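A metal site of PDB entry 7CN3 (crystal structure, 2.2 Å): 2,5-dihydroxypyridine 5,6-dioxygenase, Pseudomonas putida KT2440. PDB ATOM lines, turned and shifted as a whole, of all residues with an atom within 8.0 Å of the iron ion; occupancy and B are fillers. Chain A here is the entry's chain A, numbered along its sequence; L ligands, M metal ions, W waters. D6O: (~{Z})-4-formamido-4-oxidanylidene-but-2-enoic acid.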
ATOM      1  N   THR A  73       8.585  -9.307  12.442  1.00  0.00           N
ATOM      2  CA  THR A  73       9.231  -8.033  12.738  1.00  0.00           C
ATOM      3  C   THR A  73       8.287  -6.852  12.627  1.00  0.00           C
ATOM      4  O   THR A  73       8.704  -5.728  12.954  1.00  0.00           O
ATOM      5  CB  THR A  73      10.414  -7.752  11.795  1.00  0.00           C
ATOM      6  OG1 THR A  73       9.903  -7.429  10.484  1.00  0.00           O
ATOM      7  CG2 THR A  73      11.335  -8.948  11.715  1.00  0.00           C
ATOM      8  N   CYS A  76       5.998  -5.175  17.162  1.00  0.00           N
ATOM      9  CA  CYS A  76       6.787  -5.438  18.382  1.00  0.00           C
ATOM     10  C   CYS A  76       5.969  -5.035  19.602  1.00  0.00           C
ATOM     11  O   CYS A  76       6.040  -3.904  20.084  1.00  0.00           O
ATOM     12  CB  CYS A  76       8.130  -4.724  18.337  1.00  0.00           C
ATOM     13  SG  CYS A  76       8.921  -4.686  16.723  1.00  0.00           S
ATOM     14  N   HIS A 105      13.009  -8.357  20.492  1.00  0.00           N
ATOM     15  CA  HIS A 105      13.822  -7.706  21.508  1.00  0.00           C
ATOM     16  C   HIS A 105      12.897  -7.165  22.584  1.00  0.00           C
ATOM     17  O   HIS A 105      12.158  -6.194  22.360  1.00  0.00           O
ATOM     18  CB  HIS A 105      14.712  -6.649  20.864  1.00  0.00           C
ATOM     19  CG  HIS A 105      15.762  -7.234  19.973  1.00  0.00           C
ATOM     20  ND1 HIS A 105      16.683  -8.151  20.409  1.00  0.00           N
ATOM     21  CD2 HIS A 105      16.009  -7.052  18.645  1.00  0.00           C
ATOM     22  CE1 HIS A 105      17.469  -8.504  19.409  1.00  0.00           C
ATOM     23  NE2 HIS A 105      17.081  -7.857  18.333  1.00  0.00           N
ATOM     24  N   PHE A 196      24.914  -1.388  13.753  1.00  0.00           N
ATOM     25  CA  PHE A 196      24.090  -0.175  13.860  1.00  0.00           C
ATOM     26  C   PHE A 196      24.212   0.429  15.248  1.00  0.00           C
ATOM     27  O   PHE A 196      24.690  -0.203  16.197  1.00  0.00           O
ATOM     28  CB  PHE A 196      22.615  -0.467  13.544  1.00  0.00           C
ATOM     29  CG  PHE A 196      22.067  -1.655  14.256  1.00  0.00           C
ATOM     30  CD1 PHE A 196      22.110  -2.918  13.672  1.00  0.00           C
ATOM     31  CD2 PHE A 196      21.530  -1.513  15.530  1.00  0.00           C
ATOM     32  CE1 PHE A 196      21.599  -4.036  14.340  1.00  0.00           C
ATOM     33  CE2 PHE A 196      21.018  -2.624  16.209  1.00  0.00           C
ATOM     34  CZ  PHE A 196      21.054  -3.893  15.603  1.00  0.00           C
ATOM     35  N   TRP A 198      22.152   4.130  17.476  1.00  0.00           N
ATOM     36  CA  TRP A 198      20.928   4.923  17.578  1.00  0.00           C
ATOM     37  C   TRP A 198      21.272   6.402  17.684  1.00  0.00           C
ATOM     38  O   TRP A 198      22.255   6.759  18.330  1.00  0.00           O
ATOM     39  CB  TRP A 198      20.105   4.519  18.809  1.00  0.00           C
ATOM     40  CG  TRP A 198      19.323   3.232  18.685  1.00  0.00           C
ATOM     41  CD1 TRP A 198      17.982   3.112  18.442  1.00  0.00           C
ATOM     42  CD2 TRP A 198      19.825   1.908  18.827  1.00  0.00           C
ATOM     43  NE1 TRP A 198      17.620   1.780  18.413  1.00  0.00           N
ATOM     44  CE2 TRP A 198      18.733   1.023  18.661  1.00  0.00           C
ATOM     45  CE3 TRP A 198      21.092   1.373  19.089  1.00  0.00           C
ATOM     46  CZ2 TRP A 198      18.880  -0.364  18.738  1.00  0.00           C
ATOM     47  CZ3 TRP A 198      21.229  -0.004  19.166  1.00  0.00           C
ATOM     48  CH2 TRP A 198      20.129  -0.856  18.985  1.00  0.00           C
ATOM     49  N   LEU A 217      10.743  -2.784   4.569  1.00  0.00           N
ATOM     50  CA  LEU A 217      10.382  -3.985   5.305  1.00  0.00           C
ATOM     51  C   LEU A 217       9.464  -3.610   6.454  1.00  0.00           C
ATOM     52  O   LEU A 217       9.834  -2.764   7.276  1.00  0.00           O
ATOM     53  CB  LEU A 217      11.635  -4.676   5.854  1.00  0.00           C
ATOM     54  CG  LEU A 217      12.730  -4.978   4.818  1.00  0.00           C
ATOM     55  CD1 LEU A 217      14.009  -5.468   5.491  1.00  0.00           C
ATOM     56  CD2 LEU A 217      12.273  -5.982   3.746  1.00  0.00           C
ATOM     57  N   SER A 264      14.619   5.053  14.761  1.00  0.00           N
ATOM     58  CA  SER A 264      15.337   4.201  15.704  1.00  0.00           C
ATOM     59  C   SER A 264      16.742   3.917  15.180  1.00  0.00           C
ATOM     60  O   SER A 264      17.538   4.859  15.035  1.00  0.00           O
ATOM     61  CB  SER A 264      14.555   2.918  15.992  1.00  0.00           C
ATOM     62  OG  SER A 264      14.161   2.273  14.803  1.00  0.00           O
ATOM     63  N   HIS A 265      17.078   2.665  14.879  1.00  0.00           N
ATOM     64  CA  HIS A 265      18.489   2.364  14.662  1.00  0.00           C
ATOM     65  C   HIS A 265      18.945   2.739  13.237  1.00  0.00           C
ATOM     66  O   HIS A 265      18.165   2.798  12.289  1.00  0.00           O
ATOM     67  CB  HIS A 265      18.807   0.889  14.943  1.00  0.00           C
ATOM     68  CG  HIS A 265      18.032  -0.081  14.109  1.00  0.00           C
ATOM     69  ND1 HIS A 265      18.395  -0.425  12.822  1.00  0.00           N
ATOM     70  CD2 HIS A 265      16.936  -0.829  14.400  1.00  0.00           C
ATOM     71  CE1 HIS A 265      17.540  -1.300  12.343  1.00  0.00           C
ATOM     72  NE2 HIS A 265      16.651  -1.577  13.279  1.00  0.00           N
ATOM     73  N   ILE A 266      20.260   2.968  13.116  1.00  0.00           N
ATOM     74  CA  ILE A 266      20.920   3.447  11.906  1.00  0.00           C
ATOM     75  C   ILE A 266      22.307   2.807  11.816  1.00  0.00           C
ATOM     76  O   ILE A 266      23.006   2.664  12.829  1.00  0.00           O
ATOM     77  CB  ILE A 266      21.040   4.989  11.888  1.00  0.00           C
ATOM     78  CG1 ILE A 266      21.787   5.475  13.130  1.00  0.00           C
ATOM     79  CG2 ILE A 266      19.659   5.683  11.804  1.00  0.00           C
ATOM     80  CD1 ILE A 266      21.954   6.969  13.203  1.00  0.00           C
ATOM     81  N   ARG A 293      18.347  -6.381   4.739  1.00  0.00           N
ATOM     82  CA  ARG A 293      18.920  -5.666   5.886  1.00  0.00           C
ATOM     83  C   ARG A 293      20.445  -5.640   5.830  1.00  0.00           C
ATOM     84  O   ARG A 293      21.077  -4.655   6.255  1.00  0.00           O
ATOM     85  CB  ARG A 293      18.456  -6.295   7.199  1.00  0.00           C
ATOM     86  CG  ARG A 293      16.990  -5.995   7.583  1.00  0.00           C
ATOM     87  CD  ARG A 293      16.599  -6.572   8.948  1.00  0.00           C
ATOM     88  NE  ARG A 293      15.179  -6.363   9.219  1.00  0.00           N
ATOM     89  CZ  ARG A 293      14.213  -7.097   8.689  1.00  0.00           C
ATOM     90  NH1 ARG A 293      14.523  -8.114   7.894  1.00  0.00           N
ATOM     91  NH2 ARG A 293      12.926  -6.833   8.949  1.00  0.00           N
ATOM     92  N   LEU A 300      20.954   1.420   6.362  1.00  0.00           N
ATOM     93  CA  LEU A 300      19.730   0.863   6.928  1.00  0.00           C
ATOM     94  C   LEU A 300      19.285   1.750   8.080  1.00  0.00           C
ATOM     95  O   LEU A 300      20.041   1.998   9.021  1.00  0.00           O
ATOM     96  CB  LEU A 300      19.940  -0.577   7.396  1.00  0.00           C
ATOM     97  CG  LEU A 300      18.783  -1.253   8.113  1.00  0.00           C
ATOM     98  CD1 LEU A 300      17.690  -1.615   7.110  1.00  0.00           C
ATOM     99  CD2 LEU A 300      19.278  -2.511   8.874  1.00  0.00           C
ATOM    100  N   PHE A 301      18.063   2.243   7.991  1.00  0.00           N
ATOM    101  CA  PHE A 301      17.476   2.941   9.117  1.00  0.00           C
ATOM    102  C   PHE A 301      16.120   2.333   9.407  1.00  0.00           C
ATOM    103  O   PHE A 301      15.585   1.551   8.613  1.00  0.00           O
ATOM    104  CB  PHE A 301      17.365   4.449   8.883  1.00  0.00           C
ATOM    105  CG  PHE A 301      16.364   4.843   7.821  1.00  0.00           C
ATOM    106  CD1 PHE A 301      16.658   4.692   6.478  1.00  0.00           C
ATOM    107  CD2 PHE A 301      15.139   5.394   8.176  1.00  0.00           C
ATOM    108  CE1 PHE A 301      15.754   5.068   5.510  1.00  0.00           C
ATOM    109  CE2 PHE A 301      14.235   5.761   7.206  1.00  0.00           C
ATOM    110  CZ  PHE A 301      14.538   5.598   5.872  1.00  0.00           C
ATOM    111  N   SER A 302      15.567   2.734  10.542  1.00  0.00           N
ATOM    112  CA  SER A 302      14.429   2.062  11.130  1.00  0.00           C
ATOM    113  C   SER A 302      13.537   3.081  11.829  1.00  0.00           C
ATOM    114  O   SER A 302      13.974   4.173  12.214  1.00  0.00           O
ATOM    115  CB  SER A 302      14.904   0.995  12.119  1.00  0.00           C
ATOM    116  OG  SER A 302      13.877   0.070  12.326  1.00  0.00           O
ATOM    117  N   THR A 303      12.269   2.706  12.021  1.00  0.00           N
ATOM    118  CA  THR A 303      11.282   3.554  12.653  1.00  0.00           C
ATOM    119  C   THR A 303      10.629   2.794  13.790  1.00  0.00           C
ATOM    120  O   THR A 303      10.569   1.575  13.776  1.00  0.00           O
ATOM    121  CB  THR A 303      10.198   4.011  11.683  1.00  0.00           C
ATOM    122  OG1 THR A 303       9.446   2.867  11.231  1.00  0.00           O
ATOM    123  CG2 THR A 303      10.787   4.709  10.494  1.00  0.00           C
ATOM    124  N   GLY A 304      10.125   3.540  14.772  1.00  0.00           N
ATOM    125  CA  GLY A 304       9.288   2.961  15.803  1.00  0.00           C
ATOM    126  C   GLY A 304       9.968   2.786  17.146  1.00  0.00           C
ATOM    127  O   GLY A 304      10.616   3.702  17.664  1.00  0.00           O
ATOM    128  N   PRO A 305       9.844   1.587  17.723  1.00  0.00           N
ATOM    129  CA  PRO A 305      10.305   1.371  19.109  1.00  0.00           C
ATOM    130  C   PRO A 305      11.814   1.493  19.243  1.00  0.00           C
ATOM    131  O   PRO A 305      12.578   1.185  18.331  1.00  0.00           O
ATOM    132  CB  PRO A 305       9.853  -0.064  19.406  1.00  0.00           C
ATOM    133  CG  PRO A 305       9.875  -0.737  18.068  1.00  0.00           C
ATOM    134  CD  PRO A 305       9.430   0.319  17.081  1.00  0.00           C
ATOM    135  N   GLU A 308      14.420  -1.077  23.463  1.00  0.00           N
ATOM    136  CA  GLU A 308      15.471  -2.083  23.624  1.00  0.00           C
ATOM    137  C   GLU A 308      16.808  -1.473  24.021  1.00  0.00           C
ATOM    138  O   GLU A 308      17.662  -2.200  24.524  1.00  0.00           O
ATOM    139  CB  GLU A 308      15.626  -2.894  22.320  1.00  0.00           C
ATOM    140  CG  GLU A 308      16.205  -2.088  21.150  1.00  0.00           C
ATOM    141  CD  GLU A 308      16.105  -2.793  19.808  1.00  0.00           C
ATOM    142  OE1 GLU A 308      15.150  -2.515  19.040  1.00  0.00           O
ATOM    143  OE2 GLU A 308      16.985  -3.620  19.494  1.00  0.00           O
ATOM    144  N   HIS A 318       6.784  -0.934  13.168  1.00  0.00           N
ATOM    145  CA  HIS A 318       8.218  -1.105  13.019  1.00  0.00           C
ATOM    146  C   HIS A 318       8.581  -1.292  11.546  1.00  0.00           C
ATOM    147  O   HIS A 318       8.150  -2.257  10.918  1.00  0.00           O
ATOM    148  CB  HIS A 318       8.676  -2.311  13.825  1.00  0.00           C
ATOM    149  CG  HIS A 318      10.094  -2.683  13.554  1.00  0.00           C
ATOM    150  ND1 HIS A 318      10.458  -3.672  12.669  1.00  0.00           N
ATOM    151  CD2 HIS A 318      11.246  -2.151  14.033  1.00  0.00           C
ATOM    152  CE1 HIS A 318      11.776  -3.754  12.634  1.00  0.00           C
ATOM    153  NE2 HIS A 318      12.268  -2.846  13.456  1.00  0.00           N
ATOM    154  N   LEU A 319       9.429  -0.412  11.027  1.00  0.00           N
ATOM    155  CA  LEU A 319       9.880  -0.525   9.653  1.00  0.00           C
ATOM    156  C   LEU A 319      11.401  -0.593   9.609  1.00  0.00           C
ATOM    157  O   LEU A 319      12.087   0.080  10.395  1.00  0.00           O
ATOM    158  CB  LEU A 319       9.378   0.659   8.795  1.00  0.00           C
ATOM    159  CG  LEU A 319       7.877   0.983   8.942  1.00  0.00           C
ATOM    160  CD1 LEU A 319       7.556   2.339   8.319  1.00  0.00           C
ATOM    161  CD2 LEU A 319       6.989  -0.119   8.312  1.00  0.00           C
ATOM    162  N   ASP A 320      11.927  -1.442   8.744  1.00  0.00           N
ATOM    163  CA  ASP A 320      13.342  -1.454   8.397  1.00  0.00           C
ATOM    164  C   ASP A 320      13.470  -1.046   6.940  1.00  0.00           C
ATOM    165  O   ASP A 320      12.808  -1.632   6.072  1.00  0.00           O
ATOM    166  CB  ASP A 320      13.961  -2.834   8.628  1.00  0.00           C
ATOM    167  CG  ASP A 320      14.260  -3.086  10.086  1.00  0.00           C
ATOM    168  OD1 ASP A 320      14.446  -2.100  10.805  1.00  0.00           O
ATOM    169  OD2 ASP A 320      14.299  -4.265  10.515  1.00  0.00           O
ATOM    170  N   ILE A 321      14.315  -0.050   6.669  1.00  0.00           N
ATOM    171  CA  ILE A 321      14.398   0.529   5.331  1.00  0.00           C
ATOM    172  C   ILE A 321      15.836   0.637   4.835  1.00  0.00           C
ATOM    173  O   ILE A 321      16.568   1.552   5.261  1.00  0.00           O
ATOM    174  CB  ILE A 321      13.739   1.922   5.302  1.00  0.00           C
ATOM    175  CG1 ILE A 321      12.256   1.814   5.688  1.00  0.00           C
ATOM    176  CG2 ILE A 321      13.920   2.569   3.929  1.00  0.00           C
ATOM    177  CD1 ILE A 321      11.520   3.146   5.760  1.00  0.00           C
HETATM  178  OB  D6O L   1      15.257  -8.429  14.897  1.00  0.00           O
HETATM  179  CG  D6O L   1      15.022  -7.839  13.802  1.00  0.00           C
HETATM  180  NE1 D6O L   1      17.710  -6.988  12.728  1.00  0.00           N
HETATM  181  CZ  D6O L   1      17.599  -8.313  12.572  1.00  0.00           C
HETATM  182  OH  D6O L   1      18.463  -9.151  12.851  1.00  0.00           O
HETATM  183  CE2 D6O L   1      16.343  -8.803  11.974  1.00  0.00           C
HETATM  184  CD2 D6O L   1      15.152  -8.588  12.547  1.00  0.00           C
HETATM  185  CG1 D6O L   1      18.307  -6.383  13.765  1.00  0.00           C
HETATM  186  OB1 D6O L   1      18.002  -6.636  14.926  1.00  0.00           O
HETATM  187  OB2 D6O L   1      14.679  -6.628  13.734  1.00  0.00           O
HETATM  188 FE    FE M   1      14.438  -2.120  13.073  1.00  0.00          FE
HETATM  189  O   HOH W   1      15.256  -4.336  12.887  1.00  0.00           O
HETATM  190  O   HOH W   2      13.946  -1.785  15.316  1.00  0.00           O
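Water W1 lies within hydrogen-bond range of an oxygen (OB2) of the ligand and the side-chain carboxylate (OD2) of Asp 320.
Within 4 Å of the iron ion: His 265, Ser 302, His 318 and Asp 320.
The guanidinium group of Arg 293 is in salt-bridge range of the side-chain carboxylate of Asp 320.
O of Asp 320 lies within hydrogen-bond range of N of Leu 217.
A ring nitrogen (ND1) of His 318 lies within hydrogen-bond range of the backbone carbonyl oxygen (O) of Thr 73, at 2.7 Å.
OG of Ser 302 lies close to O of Leu 319, 2.6 Å away.
N of Ser 264 sits at hydrogen-bond distance from O of Ser 302, at 2.8 Å.
The iron ion is bound by OD1 of Asp 320, NE2 of His 265, NE2 of His 318, water W2, water W1 and OG of Ser 302.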
